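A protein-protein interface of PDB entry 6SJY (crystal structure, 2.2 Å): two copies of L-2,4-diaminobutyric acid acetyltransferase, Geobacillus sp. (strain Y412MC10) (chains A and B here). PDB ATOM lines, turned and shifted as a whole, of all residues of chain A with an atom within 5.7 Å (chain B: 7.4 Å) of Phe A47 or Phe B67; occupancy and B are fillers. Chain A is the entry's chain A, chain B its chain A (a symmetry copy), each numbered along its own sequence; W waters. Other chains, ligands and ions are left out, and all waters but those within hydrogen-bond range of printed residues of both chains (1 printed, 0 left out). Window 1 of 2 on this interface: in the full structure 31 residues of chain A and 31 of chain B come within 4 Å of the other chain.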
ATOM      1  N   LEU A  42      -8.185 -11.365   1.549  1.00  0.00           N
ATOM      2  CA  LEU A  42      -7.943 -12.045   0.312  1.00  0.00           C
ATOM      3  C   LEU A  42      -7.286 -11.165  -0.707  1.00  0.00           C
ATOM      4  O   LEU A  42      -6.511 -11.650  -1.528  1.00  0.00           O
ATOM      5  CB  LEU A  42      -9.247 -12.485  -0.332  1.00  0.00           C
ATOM      6  CG  LEU A  42     -10.007 -13.677   0.128  1.00  0.00           C
ATOM      7  CD1 LEU A  42     -11.210 -13.878  -0.804  1.00  0.00           C
ATOM      8  CD2 LEU A  42      -9.136 -14.945   0.275  1.00  0.00           C
ATOM      9  N   LEU A  43      -7.661  -9.884  -0.743  1.00  0.00           N
ATOM     10  CA  LEU A  43      -6.979  -8.976  -1.665  1.00  0.00           C
ATOM     11  C   LEU A  43      -5.490  -8.847  -1.291  1.00  0.00           C
ATOM     12  O   LEU A  43      -4.644  -8.960  -2.154  1.00  0.00           O
ATOM     13  CB  LEU A  43      -7.625  -7.584  -1.677  1.00  0.00           C
ATOM     14  CG  LEU A  43      -9.025  -7.527  -2.316  1.00  0.00           C
ATOM     15  CD1 LEU A  43      -9.602  -6.163  -2.021  1.00  0.00           C
ATOM     16  CD2 LEU A  43      -8.979  -7.808  -3.819  1.00  0.00           C
ATOM     17  N   GLY A  44      -5.186  -8.720   0.003  1.00  0.00           N
ATOM     18  CA  GLY A  44      -3.775  -8.746   0.447  1.00  0.00           C
ATOM     19  C   GLY A  44      -3.061 -10.059   0.108  1.00  0.00           C
ATOM     20  O   GLY A  44      -1.874 -10.102  -0.141  1.00  0.00           O
ATOM     21  N   ASP A  45      -3.810 -11.141   0.023  1.00  0.00           N
ATOM     22  CA  ASP A  45      -3.222 -12.469  -0.144  1.00  0.00           C
ATOM     23  C   ASP A  45      -3.041 -12.807  -1.607  1.00  0.00           C
ATOM     24  O   ASP A  45      -1.937 -13.188  -2.008  1.00  0.00           O
ATOM     25  CB  ASP A  45      -4.149 -13.493   0.547  1.00  0.00           C
ATOM     26  CG  ASP A  45      -3.409 -14.773   1.050  1.00  0.00           C
ATOM     27  OD1 ASP A  45      -2.249 -14.974   0.732  1.00  0.00           O
ATOM     28  OD2 ASP A  45      -4.050 -15.576   1.782  1.00  0.00           O
ATOM     29  N   TYR A  46      -4.132 -12.710  -2.394  1.00  0.00           N
ATOM     30  CA  TYR A  46      -4.126 -13.192  -3.750  1.00  0.00           C
ATOM     31  C   TYR A  46      -4.042 -12.091  -4.782  1.00  0.00           C
ATOM     32  O   TYR A  46      -3.618 -12.353  -5.953  1.00  0.00           O
ATOM     33  CB  TYR A  46      -5.376 -14.031  -4.046  1.00  0.00           C
ATOM     34  CG  TYR A  46      -5.401 -15.296  -3.270  1.00  0.00           C
ATOM     35  CD1 TYR A  46      -4.748 -16.438  -3.750  1.00  0.00           C
ATOM     36  CD2 TYR A  46      -6.075 -15.381  -2.065  1.00  0.00           C
ATOM     37  CE1 TYR A  46      -4.754 -17.631  -3.043  1.00  0.00           C
ATOM     38  CE2 TYR A  46      -6.115 -16.568  -1.339  1.00  0.00           C
ATOM     39  CZ  TYR A  46      -5.423 -17.682  -1.814  1.00  0.00           C
ATOM     40  OH  TYR A  46      -5.444 -18.867  -1.119  1.00  0.00           O
ATOM     41  N   PHE A  47      -4.460 -10.887  -4.429  1.00  0.00           N
ATOM     42  CA  PHE A  47      -4.441  -9.828  -5.471  1.00  0.00           C
ATOM     43  C   PHE A  47      -3.423  -8.745  -5.209  1.00  0.00           C
ATOM     44  O   PHE A  47      -3.490  -7.657  -5.801  1.00  0.00           O
ATOM     45  CB  PHE A  47      -5.822  -9.213  -5.615  1.00  0.00           C
ATOM     46  CG  PHE A  47      -6.857 -10.173  -6.179  1.00  0.00           C
ATOM     47  CD1 PHE A  47      -7.592 -10.960  -5.343  1.00  0.00           C
ATOM     48  CD2 PHE A  47      -7.051 -10.282  -7.536  1.00  0.00           C
ATOM     49  CE1 PHE A  47      -8.542 -11.866  -5.852  1.00  0.00           C
ATOM     50  CE2 PHE A  47      -8.018 -11.128  -8.050  1.00  0.00           C
ATOM     51  CZ  PHE A  47      -8.753 -11.956  -7.208  1.00  0.00           C
ATOM     52  N   ASN A  48      -2.466  -9.027  -4.352  1.00  0.00           N
ATOM     53  CA  ASN A  48      -1.613  -7.968  -3.876  1.00  0.00           C
ATOM     54  C   ASN A  48      -0.666  -7.416  -4.860  1.00  0.00           C
ATOM     55  O   ASN A  48      -0.229  -6.307  -4.693  1.00  0.00           O
ATOM     56  CB  ASN A  48      -0.984  -8.243  -2.532  1.00  0.00           C
ATOM     57  CG  ASN A  48       0.142  -9.257  -2.563  1.00  0.00           C
ATOM     58  OD1 ASN A  48       0.542  -9.823  -3.563  1.00  0.00           O
ATOM     59  ND2 ASN A  48       0.661  -9.479  -1.403  1.00  0.00           N
ATOM     60  N   ASP A  49      -0.448  -8.145  -5.937  1.00  0.00           N
ATOM     61  CA  ASP A  49       0.344  -7.640  -7.017  1.00  0.00           C
ATOM     62  C   ASP A  49      -0.254  -6.455  -7.753  1.00  0.00           C
ATOM     63  O   ASP A  49       0.514  -5.690  -8.388  1.00  0.00           O
ATOM     64  CB  ASP A  49       0.640  -8.747  -8.029  1.00  0.00           C
ATOM     65  CG  ASP A  49       1.392  -9.899  -7.366  1.00  0.00           C
ATOM     66  OD1 ASP A  49       2.546  -9.655  -7.002  1.00  0.00           O
ATOM     67  OD2 ASP A  49       0.792 -10.952  -7.073  1.00  0.00           O
ATOM     68  N   THR A  50      -1.585  -6.315  -7.675  1.00  0.00           N
ATOM     69  CA  THR A  50      -2.270  -5.230  -8.321  1.00  0.00           C
ATOM     70  C   THR A  50      -3.020  -4.433  -7.347  1.00  0.00           C
ATOM     71  O   THR A  50      -4.065  -3.878  -7.717  1.00  0.00           O
ATOM     72  CB  THR A  50      -3.211  -5.744  -9.400  1.00  0.00           C
ATOM     73  OG1 THR A  50      -4.183  -6.630  -8.828  1.00  0.00           O
ATOM     74  CG2 THR A  50      -2.463  -6.460 -10.417  1.00  0.00           C
ATOM     75  N   CYS A  51      -2.527  -4.358  -6.110  1.00  0.00           N
ATOM     76  CA  CYS A  51      -3.112  -3.469  -5.099  1.00  0.00           C
ATOM     77  C   CYS A  51      -1.998  -2.667  -4.453  1.00  0.00           C
ATOM     78  O   CYS A  51      -0.829  -3.049  -4.567  1.00  0.00           O
ATOM     79  CB  CYS A  51      -3.849  -4.188  -3.984  1.00  0.00           C
ATOM     80  SG  CYS A  51      -5.245  -5.247  -4.512  1.00  0.00           S
ATOM     81  N   ALA A  66      -7.210  -3.519  -7.240  1.00  0.00           N
ATOM     82  CA  ALA A  66      -7.485  -3.716  -8.618  1.00  0.00           C
ATOM     83  C   ALA A  66      -7.192  -5.148  -8.960  1.00  0.00           C
ATOM     84  O   ALA A  66      -6.507  -5.827  -8.203  1.00  0.00           O
ATOM     85  CB  ALA A  66      -6.594  -2.801  -9.465  1.00  0.00           C
ATOM     86  N   PHE A  67      -7.701  -5.597 -10.086  1.00  0.00           N
ATOM     87  CA  PHE A  67      -7.364  -6.911 -10.619  1.00  0.00           C
ATOM     88  C   PHE A  67      -7.375  -6.848 -12.106  1.00  0.00           C
ATOM     89  O   PHE A  67      -8.082  -6.048 -12.670  1.00  0.00           O
ATOM     90  CB  PHE A  67      -8.403  -7.941 -10.181  1.00  0.00           C
ATOM     91  CG  PHE A  67      -9.848  -7.570 -10.478  1.00  0.00           C
ATOM     92  CD1 PHE A  67     -10.451  -7.961 -11.686  1.00  0.00           C
ATOM     93  CD2 PHE A  67     -10.620  -6.929  -9.543  1.00  0.00           C
ATOM     94  CE1 PHE A  67     -11.787  -7.710 -11.956  1.00  0.00           C
ATOM     95  CE2 PHE A  67     -11.943  -6.648  -9.807  1.00  0.00           C
ATOM     96  CZ  PHE A  67     -12.537  -7.019 -11.027  1.00  0.00           C
ATOM     97  N   LEU B  43     -18.461  -9.695  -9.212  1.00  0.00           N
ATOM     98  CA  LEU B  43     -18.256 -11.126  -9.435  1.00  0.00           C
ATOM     99  C   LEU B  43     -19.124 -11.619 -10.607  1.00  0.00           C
ATOM    100  O   LEU B  43     -18.623 -12.299 -11.479  1.00  0.00           O
ATOM    101  CB  LEU B  43     -18.573 -11.950  -8.181  1.00  0.00           C
ATOM    102  CG  LEU B  43     -17.579 -11.768  -7.019  1.00  0.00           C
ATOM    103  CD1 LEU B  43     -18.173 -12.444  -5.805  1.00  0.00           C
ATOM    104  CD2 LEU B  43     -16.196 -12.328  -7.356  1.00  0.00           C
ATOM    105  N   PHE B  47     -15.981 -12.035 -12.847  1.00  0.00           N
ATOM    106  CA  PHE B  47     -15.508 -13.383 -12.438  1.00  0.00           C
ATOM    107  C   PHE B  47     -16.498 -14.482 -12.737  1.00  0.00           C
ATOM    108  O   PHE B  47     -16.393 -15.593 -12.192  1.00  0.00           O
ATOM    109  CB  PHE B  47     -15.163 -13.388 -10.959  1.00  0.00           C
ATOM    110  CG  PHE B  47     -13.958 -12.528 -10.615  1.00  0.00           C
ATOM    111  CD1 PHE B  47     -14.120 -11.214 -10.294  1.00  0.00           C
ATOM    112  CD2 PHE B  47     -12.687 -13.053 -10.646  1.00  0.00           C
ATOM    113  CE1 PHE B  47     -13.011 -10.401  -9.990  1.00  0.00           C
ATOM    114  CE2 PHE B  47     -11.592 -12.283 -10.297  1.00  0.00           C
ATOM    115  CZ  PHE B  47     -11.743 -10.933  -9.996  1.00  0.00           C
ATOM    116  N   THR B  50     -15.950 -18.316 -13.344  1.00  0.00           N
ATOM    117  CA  THR B  50     -15.591 -19.209 -12.278  1.00  0.00           C
ATOM    118  C   THR B  50     -16.488 -19.038 -11.132  1.00  0.00           C
ATOM    119  O   THR B  50     -16.038 -19.243  -9.994  1.00  0.00           O
ATOM    120  CB  THR B  50     -14.150 -18.989 -11.843  1.00  0.00           C
ATOM    121  OG1 THR B  50     -13.969 -17.638 -11.397  1.00  0.00           O
ATOM    122  CG2 THR B  50     -13.249 -19.243 -12.951  1.00  0.00           C
ATOM    123  N   CYS B  51     -17.742 -18.664 -11.387  1.00  0.00           N
ATOM    124  CA  CYS B  51     -18.761 -18.609 -10.331  1.00  0.00           C
ATOM    125  C   CYS B  51     -20.002 -19.338 -10.815  1.00  0.00           C
ATOM    126  O   CYS B  51     -20.146 -19.558 -12.021  1.00  0.00           O
ATOM    127  CB  CYS B  51     -19.189 -17.205  -9.946  1.00  0.00           C
ATOM    128  SG  CYS B  51     -17.855 -16.110  -9.338  1.00  0.00           S
ATOM    129  N   SER B  65     -18.629 -18.549  -5.435  1.00  0.00           N
ATOM    130  CA  SER B  65     -17.671 -17.637  -6.065  1.00  0.00           C
ATOM    131  C   SER B  65     -16.294 -18.240  -6.001  1.00  0.00           C
ATOM    132  O   SER B  65     -15.913 -18.821  -4.984  1.00  0.00           O
ATOM    133  CB  SER B  65     -17.613 -16.306  -5.336  1.00  0.00           C
ATOM    134  OG  SER B  65     -17.509 -16.364  -3.911  1.00  0.00           O
ATOM    135  N   ALA B  66     -15.535 -18.048  -7.067  1.00  0.00           N
ATOM    136  CA  ALA B  66     -14.184 -18.483  -7.075  1.00  0.00           C
ATOM    137  C   ALA B  66     -13.429 -17.668  -8.084  1.00  0.00           C
ATOM    138  O   ALA B  66     -14.041 -17.031  -8.934  1.00  0.00           O
ATOM    139  CB  ALA B  66     -14.114 -19.963  -7.465  1.00  0.00           C
ATOM    140  N   PHE B  67     -12.117 -17.691  -7.991  1.00  0.00           N
ATOM    141  CA  PHE B  67     -11.259 -17.080  -8.998  1.00  0.00           C
ATOM    142  C   PHE B  67     -10.005 -17.875  -9.113  1.00  0.00           C
ATOM    143  O   PHE B  67      -9.599 -18.497  -8.162  1.00  0.00           O
ATOM    144  CB  PHE B  67     -10.883 -15.660  -8.582  1.00  0.00           C
ATOM    145  CG  PHE B  67     -10.290 -15.529  -7.187  1.00  0.00           C
ATOM    146  CD1 PHE B  67      -8.900 -15.602  -6.994  1.00  0.00           C
ATOM    147  CD2 PHE B  67     -11.084 -15.249  -6.104  1.00  0.00           C
ATOM    148  CE1 PHE B  67      -8.319 -15.408  -5.750  1.00  0.00           C
ATOM    149  CE2 PHE B  67     -10.526 -15.081  -4.857  1.00  0.00           C
ATOM    150  CZ  PHE B  67      -9.135 -15.178  -4.662  1.00  0.00           C
ATOM    151  N   ARG B  68      -9.367 -17.758 -10.254  1.00  0.00           N
ATOM    152  CA  ARG B  68      -8.054 -18.214 -10.485  1.00  0.00           C
ATOM    153  C   ARG B  68      -7.039 -17.318  -9.953  1.00  0.00           C
ATOM    154  O   ARG B  68      -7.070 -16.127 -10.177  1.00  0.00           O
ATOM    155  CB  ARG B  68      -7.802 -18.496 -11.930  1.00  0.00           C
ATOM    156  CG  ARG B  68      -8.785 -19.576 -12.364  1.00  0.00           C
ATOM    157  CD  ARG B  68      -8.643 -20.050 -13.785  1.00  0.00           C
ATOM    158  NE  ARG B  68      -7.490 -20.886 -13.976  1.00  0.00           N
ATOM    159  CZ  ARG B  68      -7.372 -21.835 -14.906  1.00  0.00           C
ATOM    160  NH1 ARG B  68      -8.385 -22.162 -15.728  1.00  0.00           N
ATOM    161  NH2 ARG B  68      -6.229 -22.504 -14.977  1.00  0.00           N
ATOM    162  N   SER B  69      -6.152 -17.888  -9.158  1.00  0.00           N
ATOM    163  CA  SER B  69      -5.187 -17.098  -8.469  1.00  0.00           C
ATOM    164  C   SER B  69      -4.289 -16.329  -9.471  1.00  0.00           C
ATOM    165  O   SER B  69      -3.573 -16.957 -10.258  1.00  0.00           O
ATOM    166  CB  SER B  69      -4.281 -17.960  -7.599  1.00  0.00           C
ATOM    167  OG  SER B  69      -3.255 -17.141  -7.133  1.00  0.00           O
ATOM    168  N   PRO B  70      -4.265 -14.978  -9.389  1.00  0.00           N
ATOM    169  CA  PRO B  70      -3.446 -14.202 -10.387  1.00  0.00           C
ATOM    170  C   PRO B  70      -1.953 -14.594 -10.496  1.00  0.00           C
ATOM    171  O   PRO B  70      -1.448 -14.777 -11.610  1.00  0.00           O
ATOM    172  CB  PRO B  70      -3.640 -12.694  -9.939  1.00  0.00           C
ATOM    173  CG  PRO B  70      -4.967 -12.696  -9.191  1.00  0.00           C
ATOM    174  CD  PRO B  70      -5.059 -14.090  -8.523  1.00  0.00           C
ATOM    175  N   ARG B  71      -1.263 -14.715  -9.376  1.00  0.00           N
ATOM    176  CA  ARG B  71       0.117 -15.235  -9.384  1.00  0.00           C
ATOM    177  C   ARG B  71       0.274 -16.678  -9.871  1.00  0.00           C
ATOM    178  O   ARG B  71       1.253 -16.946 -10.481  1.00  0.00           O
ATOM    179  CB  ARG B  71       0.761 -15.215  -7.982  1.00  0.00           C
ATOM    180  CG  ARG B  71       1.241 -13.849  -7.624  1.00  0.00           C
ATOM    181  CD  ARG B  71       2.002 -13.720  -6.307  1.00  0.00           C
ATOM    182  NE  ARG B  71       1.194 -14.405  -5.380  1.00  0.00           N
ATOM    183  CZ  ARG B  71       0.232 -13.913  -4.608  1.00  0.00           C
ATOM    184  NH1 ARG B  71      -0.122 -12.618  -4.532  1.00  0.00           N
ATOM    185  NH2 ARG B  71      -0.392 -14.805  -3.866  1.00  0.00           N
ATOM    186  N   ASN B  72      -0.611 -17.598  -9.493  1.00  0.00           N
ATOM    187  CA  ASN B  72      -0.490 -19.037  -9.943  1.00  0.00           C
ATOM    188  C   ASN B  72      -1.846 -19.447 -10.386  1.00  0.00           C
ATOM    189  O   ASN B  72      -2.687 -19.940  -9.646  1.00  0.00           O
ATOM    190  CB  ASN B  72       0.078 -20.141  -8.993  1.00  0.00           C
ATOM    191  CG  ASN B  72      -0.021 -21.572  -9.659  1.00  0.00           C
ATOM    192  OD1 ASN B  72       0.015 -21.679 -10.931  1.00  0.00           O
ATOM    193  ND2 ASN B  72      -0.332 -22.643  -8.836  1.00  0.00           N
ATOM    194  N   PRO B  73      -2.080 -19.212 -11.669  1.00  0.00           N
ATOM    195  CA  PRO B  73      -3.428 -19.483 -12.184  1.00  0.00           C
ATOM    196  C   PRO B  73      -3.820 -20.922 -12.324  1.00  0.00           C
ATOM    197  O   PRO B  73      -4.987 -21.195 -12.640  1.00  0.00           O
ATOM    198  CB  PRO B  73      -3.435 -18.846 -13.587  1.00  0.00           C
ATOM    199  CG  PRO B  73      -2.197 -18.079 -13.694  1.00  0.00           C
ATOM    200  CD  PRO B  73      -1.213 -18.594 -12.680  1.00  0.00           C
ATOM    201  N   THR B  75      -4.051 -22.485  -9.704  1.00  0.00           N
ATOM    202  CA  THR B  75      -4.817 -22.598  -8.432  1.00  0.00           C
ATOM    203  C   THR B  75      -6.113 -21.863  -8.511  1.00  0.00           C
ATOM    204  O   THR B  75      -6.106 -20.692  -8.842  1.00  0.00           O
ATOM    205  CB  THR B  75      -3.981 -22.105  -7.249  1.00  0.00           C
ATOM    206  OG1 THR B  75      -2.873 -22.967  -7.129  1.00  0.00           O
ATOM    207  CG2 THR B  75      -4.757 -22.127  -5.950  1.00  0.00           C
ATOM    208  N   LEU B  76      -7.224 -22.572  -8.302  1.00  0.00           N
ATOM    209  CA  LEU B  76      -8.547 -21.992  -8.126  1.00  0.00           C
ATOM    210  C   LEU B  76      -8.853 -21.795  -6.682  1.00  0.00           C
ATOM    211  O   LEU B  76      -8.838 -22.767  -5.889  1.00  0.00           O
ATOM    212  CB  LEU B  76      -9.608 -22.898  -8.730  1.00  0.00           C
ATOM    213  CG  LEU B  76     -10.991 -22.297  -8.755  1.00  0.00           C
ATOM    214  CD1 LEU B  76     -11.170 -21.244  -9.876  1.00  0.00           C
ATOM    215  CD2 LEU B  76     -12.026 -23.420  -8.948  1.00  0.00           C
ATOM    216  N   PHE B  77      -9.139 -20.552  -6.298  1.00  0.00           N
ATOM    217  CA  PHE B  77      -9.554 -20.261  -4.965  1.00  0.00           C
ATOM    218  C   PHE B  77     -11.040 -20.167  -4.887  1.00  0.00           C
ATOM    219  O   PHE B  77     -11.654 -19.386  -5.639  1.00  0.00           O
ATOM    220  CB  PHE B  77      -8.929 -18.976  -4.471  1.00  0.00           C
ATOM    221  CG  PHE B  77      -9.224 -18.703  -3.056  1.00  0.00           C
ATOM    222  CD1 PHE B  77     -10.357 -18.035  -2.675  1.00  0.00           C
ATOM    223  CD2 PHE B  77      -8.372 -19.190  -2.080  1.00  0.00           C
ATOM    224  CE1 PHE B  77     -10.634 -17.846  -1.323  1.00  0.00           C
ATOM    225  CE2 PHE B  77      -8.649 -19.026  -0.725  1.00  0.00           C
ATOM    226  CZ  PHE B  77      -9.769 -18.340  -0.345  1.00  0.00           C
ATOM    227  N   VAL B  78     -11.641 -20.950  -3.988  1.00  0.00           N
ATOM    228  CA  VAL B  78     -13.073 -20.896  -3.758  1.00  0.00           C
ATOM    229  C   VAL B  78     -13.301 -20.031  -2.560  1.00  0.00           C
ATOM    230  O   VAL B  78     -12.844 -20.304  -1.461  1.00  0.00           O
ATOM    231  CB  VAL B  78     -13.711 -22.267  -3.587  1.00  0.00           C
ATOM    232  CG1 VAL B  78     -15.191 -22.136  -3.231  1.00  0.00           C
ATOM    233  CG2 VAL B  78     -13.494 -23.058  -4.845  1.00  0.00           C
ATOM    234  N   TRP B  79     -13.985 -18.937  -2.830  1.00  0.00           N
ATOM    235  CA  TRP B  79     -14.220 -17.857  -1.914  1.00  0.00           C
ATOM    236  C   TRP B  79     -15.460 -18.122  -1.083  1.00  0.00           C
ATOM    237  O   TRP B  79     -15.316 -18.254   0.070  1.00  0.00           O
ATOM    238  CB  TRP B  79     -14.329 -16.517  -2.689  1.00  0.00           C
ATOM    239  CG  TRP B  79     -14.511 -15.266  -1.865  1.00  0.00           C
ATOM    240  CD1 TRP B  79     -14.724 -15.142  -0.499  1.00  0.00           C
ATOM    241  CD2 TRP B  79     -14.517 -13.952  -2.379  1.00  0.00           C
ATOM    242  NE1 TRP B  79     -14.872 -13.816  -0.170  1.00  0.00           N
ATOM    243  CE2 TRP B  79     -14.744 -13.078  -1.311  1.00  0.00           C
ATOM    244  CE3 TRP B  79     -14.306 -13.419  -3.651  1.00  0.00           C
ATOM    245  CZ2 TRP B  79     -14.760 -11.733  -1.478  1.00  0.00           C
ATOM    246  CZ3 TRP B  79     -14.363 -12.066  -3.815  1.00  0.00           C
ATOM    247  CH2 TRP B  79     -14.579 -11.245  -2.748  1.00  0.00           C
ATOM    248  N   LEU B 100     -19.024 -26.091 -11.200  1.00  0.00           N
ATOM    249  CA  LEU B 100     -17.948 -25.121 -11.284  1.00  0.00           C
ATOM    250  C   LEU B 100     -16.730 -25.764 -11.886  1.00  0.00           C
ATOM    251  O   LEU B 100     -16.147 -25.198 -12.833  1.00  0.00           O
ATOM    252  CB  LEU B 100     -17.620 -24.496  -9.908  1.00  0.00           C
ATOM    253  CG  LEU B 100     -16.375 -23.614  -9.841  1.00  0.00           C
ATOM    254  CD1 LEU B 100     -16.486 -22.414 -10.802  1.00  0.00           C
ATOM    255  CD2 LEU B 100     -16.103 -23.105  -8.441  1.00  0.00           C
ATOM    256  N   VAL B 109      -6.701 -26.206 -14.155  1.00  0.00           N
ATOM    257  CA  VAL B 109      -6.542 -26.060 -12.704  1.00  0.00           C
ATOM    258  C   VAL B 109      -5.925 -27.384 -12.145  1.00  0.00           C
ATOM    259  O   VAL B 109      -6.366 -28.432 -12.473  1.00  0.00           O
ATOM    260  CB  VAL B 109      -7.925 -25.777 -12.051  1.00  0.00           C
ATOM    261  CG1 VAL B 109      -7.925 -25.879 -10.539  1.00  0.00           C
ATOM    262  CG2 VAL B 109      -8.395 -24.345 -12.420  1.00  0.00           C
ATOM    263  N   GLU B 113      -7.967 -24.190  -3.645  1.00  0.00           N
ATOM    264  CA  GLU B 113      -7.732 -23.700  -2.276  1.00  0.00           C
ATOM    265  C   GLU B 113      -8.957 -23.010  -1.800  1.00  0.00           C
ATOM    266  O   GLU B 113      -9.708 -22.371  -2.582  1.00  0.00           O
ATOM    267  CB  GLU B 113      -6.585 -22.718  -2.183  1.00  0.00           C
ATOM    268  CG  GLU B 113      -5.281 -23.252  -2.574  1.00  0.00           C
ATOM    269  CD  GLU B 113      -4.135 -22.272  -2.326  1.00  0.00           C
ATOM    270  OE1 GLU B 113      -3.033 -22.745  -2.395  1.00  0.00           O
ATOM    271  OE2 GLU B 113      -4.300 -21.066  -2.099  1.00  0.00           O
HETATM  272  O   HOH W   1      -2.374 -14.632  -6.788  1.00  0.00           O
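O of Asp A45 lies within hydrogen-bond range of NH2 of Arg B71. The side-chain carboxylate (OD2) of Asp A49 is in salt-bridge range of the guanidinium group (NH1) of Arg B71 (3.2 Å). OH of Tyr A46 is in hydrogen-bond range of OE2 of Glu B113. The guanidinium group of Arg B71 sits at hydrogen-bond distance from the side-chain amide oxygen of Asn A48, at 3.0 Å.
The backbone NH of Ser B69 is in hydrogen-bond range of the backbone carbonyl oxygen of Thr B75 (2.8 Å). O of Leu A43 is in hydrogen-bond range of N of Asn A48 (3.1 Å). The backbone carbonyl oxygen of Phe B47 lies within hydrogen-bond range of the side-chain hydroxyl of Thr B50 (3.3 Å). The backbone carbonyl oxygen (O) of Ser B65 sits at hydrogen-bond distance from the backbone NH (N) of Trp B79 (2.9 Å). The backbone carbonyl oxygen (O) of Phe A47 lies within hydrogen-bond range of the side-chain sulfur (SG) of Cys A51 (3.2 Å). O of Phe B47 is in hydrogen-bond range of SG of Cys B51, at 3.2 Å.
Among the printed residues, merely in contact across the chains: Tyr A46 with Phe B77 (3.1 Å), Tyr A46 with Pro B70 (3.4 Å), Leu A42 with Phe B77 (3.5 Å), Phe A67 with Phe B47 (3.6 Å), Phe A47 with Phe B67 (3.6 Å), Phe A47 with Pro B70 (3.6 Å), Leu A42 with Trp B79 (3.7 Å), Tyr A46 with Phe B67 (3.7 Å), Tyr A46 with Ser B69 (3.8 Å) and Tyr A46 with Arg B71 (3.8 Å).
Of chain A, only Tyr A46 and Phe A47 come within 4 Å of Phe B67. Of the printed residues of chain A, Glu B113 touches Tyr A46. Of the printed residues of chain A, Ser B69 touches Tyr A46 (3.8 Å). Asn B72 touches none of the printed residues of chain A. The nearest residue of chain B that does not touch Phe A47 is Phe B47 (4.2 Å). The nearest residue of chain A that does not touch Phe B67 is Leu A42 (4.3 Å).
Along chain B the printed residues that touch a printed residue of chain A span positions 47 to 113. Printed residues of chain A that touch a printed residue of chain B: Leu A42, Asp A45, Tyr A46, Phe A47, Asn A48, Asp A49 and Phe A67. Hydrophobic or aromatic side chains of chain A within 4 Å of the printed part of chain B: Leu A42, Tyr A46, Phe A47 and Phe A67. Along chain A the printed residues that touch a printed residue of chain B span positions 42 to 67. Among the printed residues, 14 pairs touch across the chains. Among the printed residues, Asp or Glu carboxylates within 4 Å of a Lys or Arg side-chain nitrogen of the other chain: Asp A49 with Arg B71 (3.2 Å).
Phe A47 touches Phe B67, and with the chains exchanged Phe A67 touches Phe B47.
Water W1 lies within hydrogen-bond range of the side-chain hydroxyl of Ser B69, the backbone carbonyl oxygen of Tyr A46 and the backbone NH of Arg B71.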
